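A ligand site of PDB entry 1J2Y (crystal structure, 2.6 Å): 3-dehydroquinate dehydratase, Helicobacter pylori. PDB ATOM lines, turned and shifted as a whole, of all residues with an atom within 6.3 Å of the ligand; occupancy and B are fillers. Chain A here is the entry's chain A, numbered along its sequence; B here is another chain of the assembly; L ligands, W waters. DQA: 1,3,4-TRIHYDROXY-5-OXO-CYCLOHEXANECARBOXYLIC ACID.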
ATOM      1  N   ASN A  10      18.160  -0.923  19.207  1.00  0.00           N
ATOM      2  CA  ASN A  10      17.361  -1.875  19.984  1.00  0.00           C
ATOM      3  C   ASN A  10      17.397  -1.798  21.515  1.00  0.00           C
ATOM      4  O   ASN A  10      17.031  -2.755  22.193  1.00  0.00           O
ATOM      5  CB  ASN A  10      17.733  -3.287  19.533  1.00  0.00           C
ATOM      6  CG  ASN A  10      17.743  -3.413  18.020  1.00  0.00           C
ATOM      7  OD1 ASN A  10      16.684  -3.459  17.385  1.00  0.00           O
ATOM      8  ND2 ASN A  10      18.940  -3.469  17.443  1.00  0.00           N
ATOM      9  N   LEU A  11      17.826  -0.668  22.065  1.00  0.00           N
ATOM     10  CA  LEU A  11      17.904  -0.527  23.503  1.00  0.00           C
ATOM     11  C   LEU A  11      16.541  -0.381  24.169  1.00  0.00           C
ATOM     12  O   LEU A  11      16.411  -0.549  25.377  1.00  0.00           O
ATOM     13  CB  LEU A  11      18.802   0.655  23.850  1.00  0.00           C
ATOM     14  CG  LEU A  11      20.260   0.281  23.655  1.00  0.00           C
ATOM     15  CD1 LEU A  11      21.192   1.439  23.945  1.00  0.00           C
ATOM     16  CD2 LEU A  11      20.555  -0.889  24.578  1.00  0.00           C
ATOM     17  N   ARG A  17      15.458  -9.029  24.687  1.00  0.00           N
ATOM     18  CA  ARG A  17      16.826  -9.429  24.360  1.00  0.00           C
ATOM     19  C   ARG A  17      17.264 -10.560  25.266  1.00  0.00           C
ATOM     20  O   ARG A  17      16.585 -10.894  26.237  1.00  0.00           O
ATOM     21  CB  ARG A  17      17.788  -8.246  24.534  1.00  0.00           C
ATOM     22  CG  ARG A  17      17.755  -7.222  23.400  1.00  0.00           C
ATOM     23  CD  ARG A  17      18.579  -5.996  23.755  1.00  0.00           C
ATOM     24  NE  ARG A  17      19.010  -5.219  22.598  1.00  0.00           N
ATOM     25  CZ  ARG A  17      20.036  -5.559  21.819  1.00  0.00           C
ATOM     26  NH1 ARG A  17      20.722  -6.657  22.062  1.00  0.00           N
ATOM     27  NH2 ARG A  17      20.387  -4.773  20.800  1.00  0.00           N
ATOM     28  N   TYR A  22      21.656  -8.906  28.710  1.00  0.00           N
ATOM     29  CA  TYR A  22      21.000  -7.725  29.252  1.00  0.00           C
ATOM     30  C   TYR A  22      20.050  -8.026  30.423  1.00  0.00           C
ATOM     31  O   TYR A  22      19.301  -7.144  30.873  1.00  0.00           O
ATOM     32  CB  TYR A  22      20.239  -7.017  28.132  1.00  0.00           C
ATOM     33  CG  TYR A  22      21.034  -6.809  26.843  1.00  0.00           C
ATOM     34  CD1 TYR A  22      21.190  -7.842  25.907  1.00  0.00           C
ATOM     35  CD2 TYR A  22      21.606  -5.574  26.549  1.00  0.00           C
ATOM     36  CE1 TYR A  22      21.905  -7.639  24.729  1.00  0.00           C
ATOM     37  CE2 TYR A  22      22.308  -5.371  25.377  1.00  0.00           C
ATOM     38  CZ  TYR A  22      22.453  -6.393  24.466  1.00  0.00           C
ATOM     39  OH  TYR A  22      23.134  -6.135  23.296  1.00  0.00           O
ATOM     40  N   ASN A  76      24.836   5.790  24.635  1.00  0.00           N
ATOM     41  CA  ASN A  76      25.077   4.393  24.333  1.00  0.00           C
ATOM     42  C   ASN A  76      24.646   4.306  22.900  1.00  0.00           C
ATOM     43  O   ASN A  76      23.494   3.998  22.615  1.00  0.00           O
ATOM     44  CB  ASN A  76      24.196   3.475  25.166  1.00  0.00           C
ATOM     45  CG  ASN A  76      24.407   2.012  24.823  1.00  0.00           C
ATOM     46  OD1 ASN A  76      24.806   1.688  23.704  1.00  0.00           O
ATOM     47  ND2 ASN A  76      24.140   1.139  25.775  1.00  0.00           N
ATOM     48  N   PRO A  77      25.560   4.586  21.958  1.00  0.00           N
ATOM     49  CA  PRO A  77      25.132   4.497  20.562  1.00  0.00           C
ATOM     50  C   PRO A  77      24.806   3.070  20.107  1.00  0.00           C
ATOM     51  O   PRO A  77      24.331   2.843  18.988  1.00  0.00           O
ATOM     52  CB  PRO A  77      26.291   5.169  19.793  1.00  0.00           C
ATOM     53  CG  PRO A  77      27.458   5.020  20.702  1.00  0.00           C
ATOM     54  CD  PRO A  77      26.918   5.141  22.089  1.00  0.00           C
ATOM     55  N   GLY A  78      25.022   2.123  21.001  1.00  0.00           N
ATOM     56  CA  GLY A  78      24.723   0.742  20.678  1.00  0.00           C
ATOM     57  C   GLY A  78      25.478   0.274  19.456  1.00  0.00           C
ATOM     58  O   GLY A  78      26.623   0.670  19.228  1.00  0.00           O
ATOM     59  N   ALA A  79      24.821  -0.562  18.653  1.00  0.00           N
ATOM     60  CA  ALA A  79      25.442  -1.135  17.470  1.00  0.00           C
ATOM     61  C   ALA A  79      26.027  -0.121  16.481  1.00  0.00           C
ATOM     62  O   ALA A  79      26.902  -0.461  15.686  1.00  0.00           O
ATOM     63  CB  ALA A  79      24.443  -2.066  16.778  1.00  0.00           C
ATOM     64  N   PHE A  80      25.566   1.124  16.524  1.00  0.00           N
ATOM     65  CA  PHE A  80      26.077   2.158  15.625  1.00  0.00           C
ATOM     66  C   PHE A  80      27.462   2.641  16.034  1.00  0.00           C
ATOM     67  O   PHE A  80      28.135   3.326  15.255  1.00  0.00           O
ATOM     68  CB  PHE A  80      25.145   3.380  15.610  1.00  0.00           C
ATOM     69  CG  PHE A  80      23.792   3.112  15.046  1.00  0.00           C
ATOM     70  CD1 PHE A  80      23.591   2.143  14.072  1.00  0.00           C
ATOM     71  CD2 PHE A  80      22.709   3.899  15.434  1.00  0.00           C
ATOM     72  CE1 PHE A  80      22.334   1.948  13.492  1.00  0.00           C
ATOM     73  CE2 PHE A  80      21.443   3.721  14.867  1.00  0.00           C
ATOM     74  CZ  PHE A  80      21.266   2.747  13.894  1.00  0.00           C
ATOM     75  N   SER A  81      27.890   2.310  17.244  1.00  0.00           N
ATOM     76  CA  SER A  81      29.201   2.753  17.699  1.00  0.00           C
ATOM     77  C   SER A  81      30.363   2.089  16.971  1.00  0.00           C
ATOM     78  O   SER A  81      31.494   2.588  16.997  1.00  0.00           O
ATOM     79  CB  SER A  81      29.323   2.570  19.208  1.00  0.00           C
ATOM     80  OG  SER A  81      28.657   1.403  19.644  1.00  0.00           O
ATOM     81  N   HIS A  82      30.092   0.974  16.292  1.00  0.00           N
ATOM     82  CA  HIS A  82      31.152   0.273  15.586  1.00  0.00           C
ATOM     83  C   HIS A  82      31.172   0.620  14.097  1.00  0.00           C
ATOM     84  O   HIS A  82      32.151   0.324  13.397  1.00  0.00           O
ATOM     85  CB  HIS A  82      30.972  -1.232  15.743  1.00  0.00           C
ATOM     86  CG  HIS A  82      30.474  -1.623  17.097  1.00  0.00           C
ATOM     87  ND1 HIS A  82      31.219  -1.455  18.239  1.00  0.00           N
ATOM     88  CD2 HIS A  82      29.283  -2.147  17.493  1.00  0.00           C
ATOM     89  CE1 HIS A  82      30.512  -1.848  19.283  1.00  0.00           C
ATOM     90  NE2 HIS A  82      29.341  -2.276  18.856  1.00  0.00           N
ATOM     91  N   VAL A 101      28.469   4.752  27.038  1.00  0.00           N
ATOM     92  CA  VAL A 101      28.116   3.670  27.908  1.00  0.00           C
ATOM     93  C   VAL A 101      27.633   2.438  27.157  1.00  0.00           C
ATOM     94  O   VAL A 101      26.830   2.533  26.238  1.00  0.00           O
ATOM     95  CB  VAL A 101      27.007   4.138  28.911  1.00  0.00           C
ATOM     96  CG1 VAL A 101      26.391   2.964  29.607  1.00  0.00           C
ATOM     97  CG2 VAL A 101      27.623   5.059  29.928  1.00  0.00           C
ATOM     98  N   HIS A 102      28.128   1.276  27.562  1.00  0.00           N
ATOM     99  CA  HIS A 102      27.756  -0.015  26.991  1.00  0.00           C
ATOM    100  C   HIS A 102      27.368  -0.973  28.119  1.00  0.00           C
ATOM    101  O   HIS A 102      28.160  -1.229  29.025  1.00  0.00           O
ATOM    102  CB  HIS A 102      28.938  -0.612  26.206  1.00  0.00           C
ATOM    103  CG  HIS A 102      29.256   0.126  24.948  1.00  0.00           C
ATOM    104  ND1 HIS A 102      28.471   0.050  23.819  1.00  0.00           N
ATOM    105  CD2 HIS A 102      30.268   0.971  24.638  1.00  0.00           C
ATOM    106  CE1 HIS A 102      28.976   0.821  22.872  1.00  0.00           C
ATOM    107  NE2 HIS A 102      30.069   1.393  23.341  1.00  0.00           N
ATOM    108  N   LEU A 103      26.150  -1.491  28.077  1.00  0.00           N
ATOM    109  CA  LEU A 103      25.659  -2.441  29.075  1.00  0.00           C
ATOM    110  C   LEU A 103      26.582  -3.640  29.135  1.00  0.00           C
ATOM    111  O   LEU A 103      27.052  -4.044  30.196  1.00  0.00           O
ATOM    112  CB  LEU A 103      24.258  -2.913  28.714  1.00  0.00           C
ATOM    113  CG  LEU A 103      23.154  -1.860  28.726  1.00  0.00           C
ATOM    114  CD1 LEU A 103      21.828  -2.476  28.284  1.00  0.00           C
ATOM    115  CD2 LEU A 103      23.042  -1.281  30.109  1.00  0.00           C
ATOM    116  N   THR A 104      26.841  -4.225  27.969  1.00  0.00           N
ATOM    117  CA  THR A 104      27.702  -5.389  27.869  1.00  0.00           C
ATOM    118  C   THR A 104      29.136  -4.950  27.650  1.00  0.00           C
ATOM    119  O   THR A 104      29.408  -3.772  27.455  1.00  0.00           O
ATOM    120  CB  THR A 104      27.304  -6.255  26.684  1.00  0.00           C
ATOM    121  OG1 THR A 104      27.360  -5.478  25.488  1.00  0.00           O
ATOM    122  CG2 THR A 104      25.904  -6.768  26.881  1.00  0.00           C
ATOM    123  N   ASN A 105      30.041  -5.919  27.691  1.00  0.00           N
ATOM    124  CA  ASN A 105      31.475  -5.685  27.483  1.00  0.00           C
ATOM    125  C   ASN A 105      31.717  -5.971  25.998  1.00  0.00           C
ATOM    126  O   ASN A 105      31.740  -7.126  25.578  1.00  0.00           O
ATOM    127  CB  ASN A 105      32.288  -6.638  28.371  1.00  0.00           C
ATOM    128  CG  ASN A 105      33.798  -6.449  28.238  1.00  0.00           C
ATOM    129  OD1 ASN A 105      34.562  -6.871  29.113  1.00  0.00           O
ATOM    130  ND2 ASN A 105      34.234  -5.835  27.145  1.00  0.00           N
ATOM    131  N   ILE A 106      31.894  -4.925  25.188  1.00  0.00           N
ATOM    132  CA  ILE A 106      32.109  -5.118  23.756  1.00  0.00           C
ATOM    133  C   ILE A 106      33.432  -5.780  23.400  1.00  0.00           C
ATOM    134  O   ILE A 106      33.667  -6.111  22.239  1.00  0.00           O
ATOM    135  CB  ILE A 106      31.981  -3.803  22.956  1.00  0.00           C
ATOM    136  CG1 ILE A 106      32.920  -2.749  23.519  1.00  0.00           C
ATOM    137  CG2 ILE A 106      30.551  -3.345  22.994  1.00  0.00           C
ATOM    138  CD1 ILE A 106      33.113  -1.587  22.593  1.00  0.00           C
ATOM    139  N   ARG A 109      32.588 -10.032  22.842  1.00  0.00           N
ATOM    140  CA  ARG A 109      31.521 -10.518  21.991  1.00  0.00           C
ATOM    141  C   ARG A 109      32.039 -10.682  20.579  1.00  0.00           C
ATOM    142  O   ARG A 109      33.232 -10.855  20.382  1.00  0.00           O
ATOM    143  CB  ARG A 109      30.343  -9.548  22.034  1.00  0.00           C
ATOM    144  CG  ARG A 109      29.754  -9.478  23.435  1.00  0.00           C
ATOM    145  CD  ARG A 109      28.706  -8.397  23.576  1.00  0.00           C
ATOM    146  NE  ARG A 109      27.547  -8.653  22.736  1.00  0.00           N
ATOM    147  CZ  ARG A 109      26.457  -7.891  22.746  1.00  0.00           C
ATOM    148  NH1 ARG A 109      26.395  -6.848  23.552  1.00  0.00           N
ATOM    149  NH2 ARG A 109      25.444  -8.181  21.947  1.00  0.00           N
ATOM    150  N   ARG A 113      32.250  -5.980  17.332  1.00  0.00           N
ATOM    151  CA  ARG A 113      31.762  -5.103  18.388  1.00  0.00           C
ATOM    152  C   ARG A 113      32.929  -4.592  19.199  1.00  0.00           C
ATOM    153  O   ARG A 113      32.740  -3.764  20.096  1.00  0.00           O
ATOM    154  CB  ARG A 113      30.812  -5.832  19.341  1.00  0.00           C
ATOM    155  CG  ARG A 113      29.384  -5.990  18.861  1.00  0.00           C
ATOM    156  CD  ARG A 113      28.460  -6.266  20.067  1.00  0.00           C
ATOM    157  NE  ARG A 113      27.323  -7.130  19.745  1.00  0.00           N
ATOM    158  CZ  ARG A 113      26.290  -6.770  18.986  1.00  0.00           C
ATOM    159  NH1 ARG A 113      26.256  -5.564  18.473  1.00  0.00           N
ATOM    160  NH2 ARG A 113      25.315  -7.633  18.720  1.00  0.00           N
ATOM    161  N   MET A 127      31.838   0.037  29.971  1.00  0.00           N
ATOM    162  CA  MET A 127      31.202  -1.143  29.403  1.00  0.00           C
ATOM    163  C   MET A 127      31.233  -2.329  30.352  1.00  0.00           C
ATOM    164  O   MET A 127      32.162  -2.473  31.147  1.00  0.00           O
ATOM    165  CB  MET A 127      31.912  -1.560  28.104  1.00  0.00           C
ATOM    166  CG  MET A 127      33.347  -2.063  28.298  1.00  0.00           C
ATOM    167  SD  MET A 127      34.232  -2.435  26.747  1.00  0.00           S
ATOM    168  CE  MET A 127      34.703  -0.888  26.280  1.00  0.00           C
ATOM    169  N   GLY A 128      30.205  -3.179  30.281  1.00  0.00           N
ATOM    170  CA  GLY A 128      30.204  -4.354  31.117  1.00  0.00           C
ATOM    171  C   GLY A 128      29.334  -4.307  32.352  1.00  0.00           C
ATOM    172  O   GLY A 128      28.675  -5.289  32.696  1.00  0.00           O
ATOM    173  N   TYR A 134      25.319   3.559  33.599  1.00  0.00           N
ATOM    174  CA  TYR A 134      24.901   4.955  33.451  1.00  0.00           C
ATOM    175  C   TYR A 134      25.053   5.762  34.747  1.00  0.00           C
ATOM    176  O   TYR A 134      25.322   6.966  34.703  1.00  0.00           O
ATOM    177  CB  TYR A 134      23.458   5.050  32.991  1.00  0.00           C
ATOM    178  CG  TYR A 134      23.199   4.392  31.676  1.00  0.00           C
ATOM    179  CD1 TYR A 134      23.173   3.003  31.552  1.00  0.00           C
ATOM    180  CD2 TYR A 134      22.944   5.169  30.536  1.00  0.00           C
ATOM    181  CE1 TYR A 134      22.896   2.391  30.327  1.00  0.00           C
ATOM    182  CE2 TYR A 134      22.673   4.569  29.308  1.00  0.00           C
ATOM    183  CZ  TYR A 134      22.647   3.195  29.212  1.00  0.00           C
ATOM    184  OH  TYR A 134      22.398   2.618  27.995  1.00  0.00           O
ATOM    185  N   ILE B  85      24.364  -4.144  11.657  1.00  0.00           N
ATOM    186  CA  ILE B  85      24.355  -5.094  12.753  1.00  0.00           C
ATOM    187  C   ILE B  85      23.121  -4.743  13.604  1.00  0.00           C
ATOM    188  O   ILE B  85      22.616  -5.582  14.347  1.00  0.00           O
ATOM    189  CB  ILE B  85      25.689  -5.050  13.574  1.00  0.00           C
ATOM    190  CG1 ILE B  85      25.397  -4.893  15.061  1.00  0.00           C
ATOM    191  CG2 ILE B  85      26.639  -4.011  13.033  1.00  0.00           C
ATOM    192  CD1 ILE B  85      25.057  -6.203  15.745  1.00  0.00           C
ATOM    193  N   ASP B  89      20.406  -7.225  14.880  1.00  0.00           N
ATOM    194  CA  ASP B  89      20.045  -7.351  16.289  1.00  0.00           C
ATOM    195  C   ASP B  89      18.531  -7.388  16.423  1.00  0.00           C
ATOM    196  O   ASP B  89      18.006  -8.205  17.171  1.00  0.00           O
ATOM    197  CB  ASP B  89      20.621  -6.181  17.118  1.00  0.00           C
ATOM    198  CG  ASP B  89      22.088  -6.355  17.424  1.00  0.00           C
ATOM    199  OD1 ASP B  89      22.596  -7.489  17.327  1.00  0.00           O
ATOM    200  OD2 ASP B  89      22.757  -5.355  17.781  1.00  0.00           O
HETATM  201  C1  DQA L   1      25.451  -2.190  23.753  1.00  0.00           C
HETATM  202  C2  DQA L   1      26.672  -2.568  23.050  1.00  0.00           C
HETATM  203  C3  DQA L   1      26.480  -2.638  21.603  1.00  0.00           C
HETATM  204  O3  DQA L   1      27.657  -2.914  20.870  1.00  0.00           O
HETATM  205  C4  DQA L   1      25.573  -3.731  21.376  1.00  0.00           C
HETATM  206  O4  DQA L   1      25.295  -4.023  20.052  1.00  0.00           O
HETATM  207  C5  DQA L   1      24.249  -3.514  22.132  1.00  0.00           C
HETATM  208  C6  DQA L   1      24.367  -3.184  23.513  1.00  0.00           C
HETATM  209  C   DQA L   1      25.528  -2.157  25.145  1.00  0.00           C
HETATM  210  O1  DQA L   1      26.629  -2.506  25.788  1.00  0.00           O
HETATM  211  O2  DQA L   1      24.516  -1.793  25.919  1.00  0.00           O
HETATM  212  O5  DQA L   1      23.198  -3.550  21.849  1.00  0.00           O
HETATM  213  O6  DQA L   1      25.142  -0.831  23.491  1.00  0.00           O
HETATM  214  O   HOH W   1      22.166  -2.125  18.857  1.00  0.00           O
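The side-chain amide oxygen of Asn 76 lies within hydrogen-bond range of an oxygen (O6) of the ligand.
N of Thr 104 sits at hydrogen-bond distance from O1 of the ligand, 2.8 Å away.
OH of Tyr 22 is in hydrogen-bond range of O5 of the ligand, at 3.0 Å.
O3 of the ligand lies within hydrogen-bond range of NE2 of His 82.
The guanidinium group of Arg 17 sits at hydrogen-bond distance from an oxygen (O5) of the ligand (3.2 Å).
An oxygen (O1) of the ligand is in hydrogen-bond range of the backbone NH of Leu 103, at 2.5 Å.
NH1 of Arg 113 is in hydrogen-bond range of O4 of the ligand.
The side-chain hydroxyl of Thr 104 lies within hydrogen-bond range of an oxygen (O1) of the ligand, 3.1 Å away.
An oxygen (O6) of the ligand lies close to a ring nitrogen (ND1) of His 102, at 3.5 Å.
ND2 of Asn 76 sits at hydrogen-bond distance from OH of Tyr 134, 3.2 Å away.
The guanidinium group (NE) of Arg 17 lies within hydrogen-bond range of the backbone carbonyl oxygen (O) of Asn 10, at 3.2 Å.
OH of Tyr 22 is in hydrogen-bond range of NH1 of Arg 17, 2.8 Å away.
The backbone carbonyl oxygen of Thr 104 sits at hydrogen-bond distance from the backbone NH of Gly 128, at 3.0 Å.
O of Arg 113 lies close to ND1 of His 82 (3.3 Å).
OD1 of Asn 76 sits at hydrogen-bond distance from N of Gly 78 (2.7 Å).
The side-chain amide nitrogen (ND2) of Asn 76 lies close to the backbone carbonyl oxygen (O) of Val 101 (3.1 Å).
The guanidinium group (NH1) of Arg 109 is in hydrogen-bond range of the side-chain hydroxyl (OG1) of Thr 104 (2.6 Å).
Merely in contact with the ligand: Gly 78 (3.3 Å), Ile 106 (3.6 Å), Asp 89 of chain B (3.7 Å), Ala 79 (3.8 Å) and Arg 109 (3.9 Å).
Within 4 Å of the ligand: Arg 17, Tyr 22, Asn 76, Gly 78, Ala 79, His 82, His 102, Leu 103, Thr 104, Ile 106, Arg 109, Arg 113 and Asp 89 of chain B.
Water W1 lies within hydrogen-bond range of the backbone NH (N) of Ala 79 (3.1 Å), the side-chain carboxylate (OD2) of Asp 89 of chain B (3.5 Å) and an oxygen (O5) of the ligand (3.5 Å).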
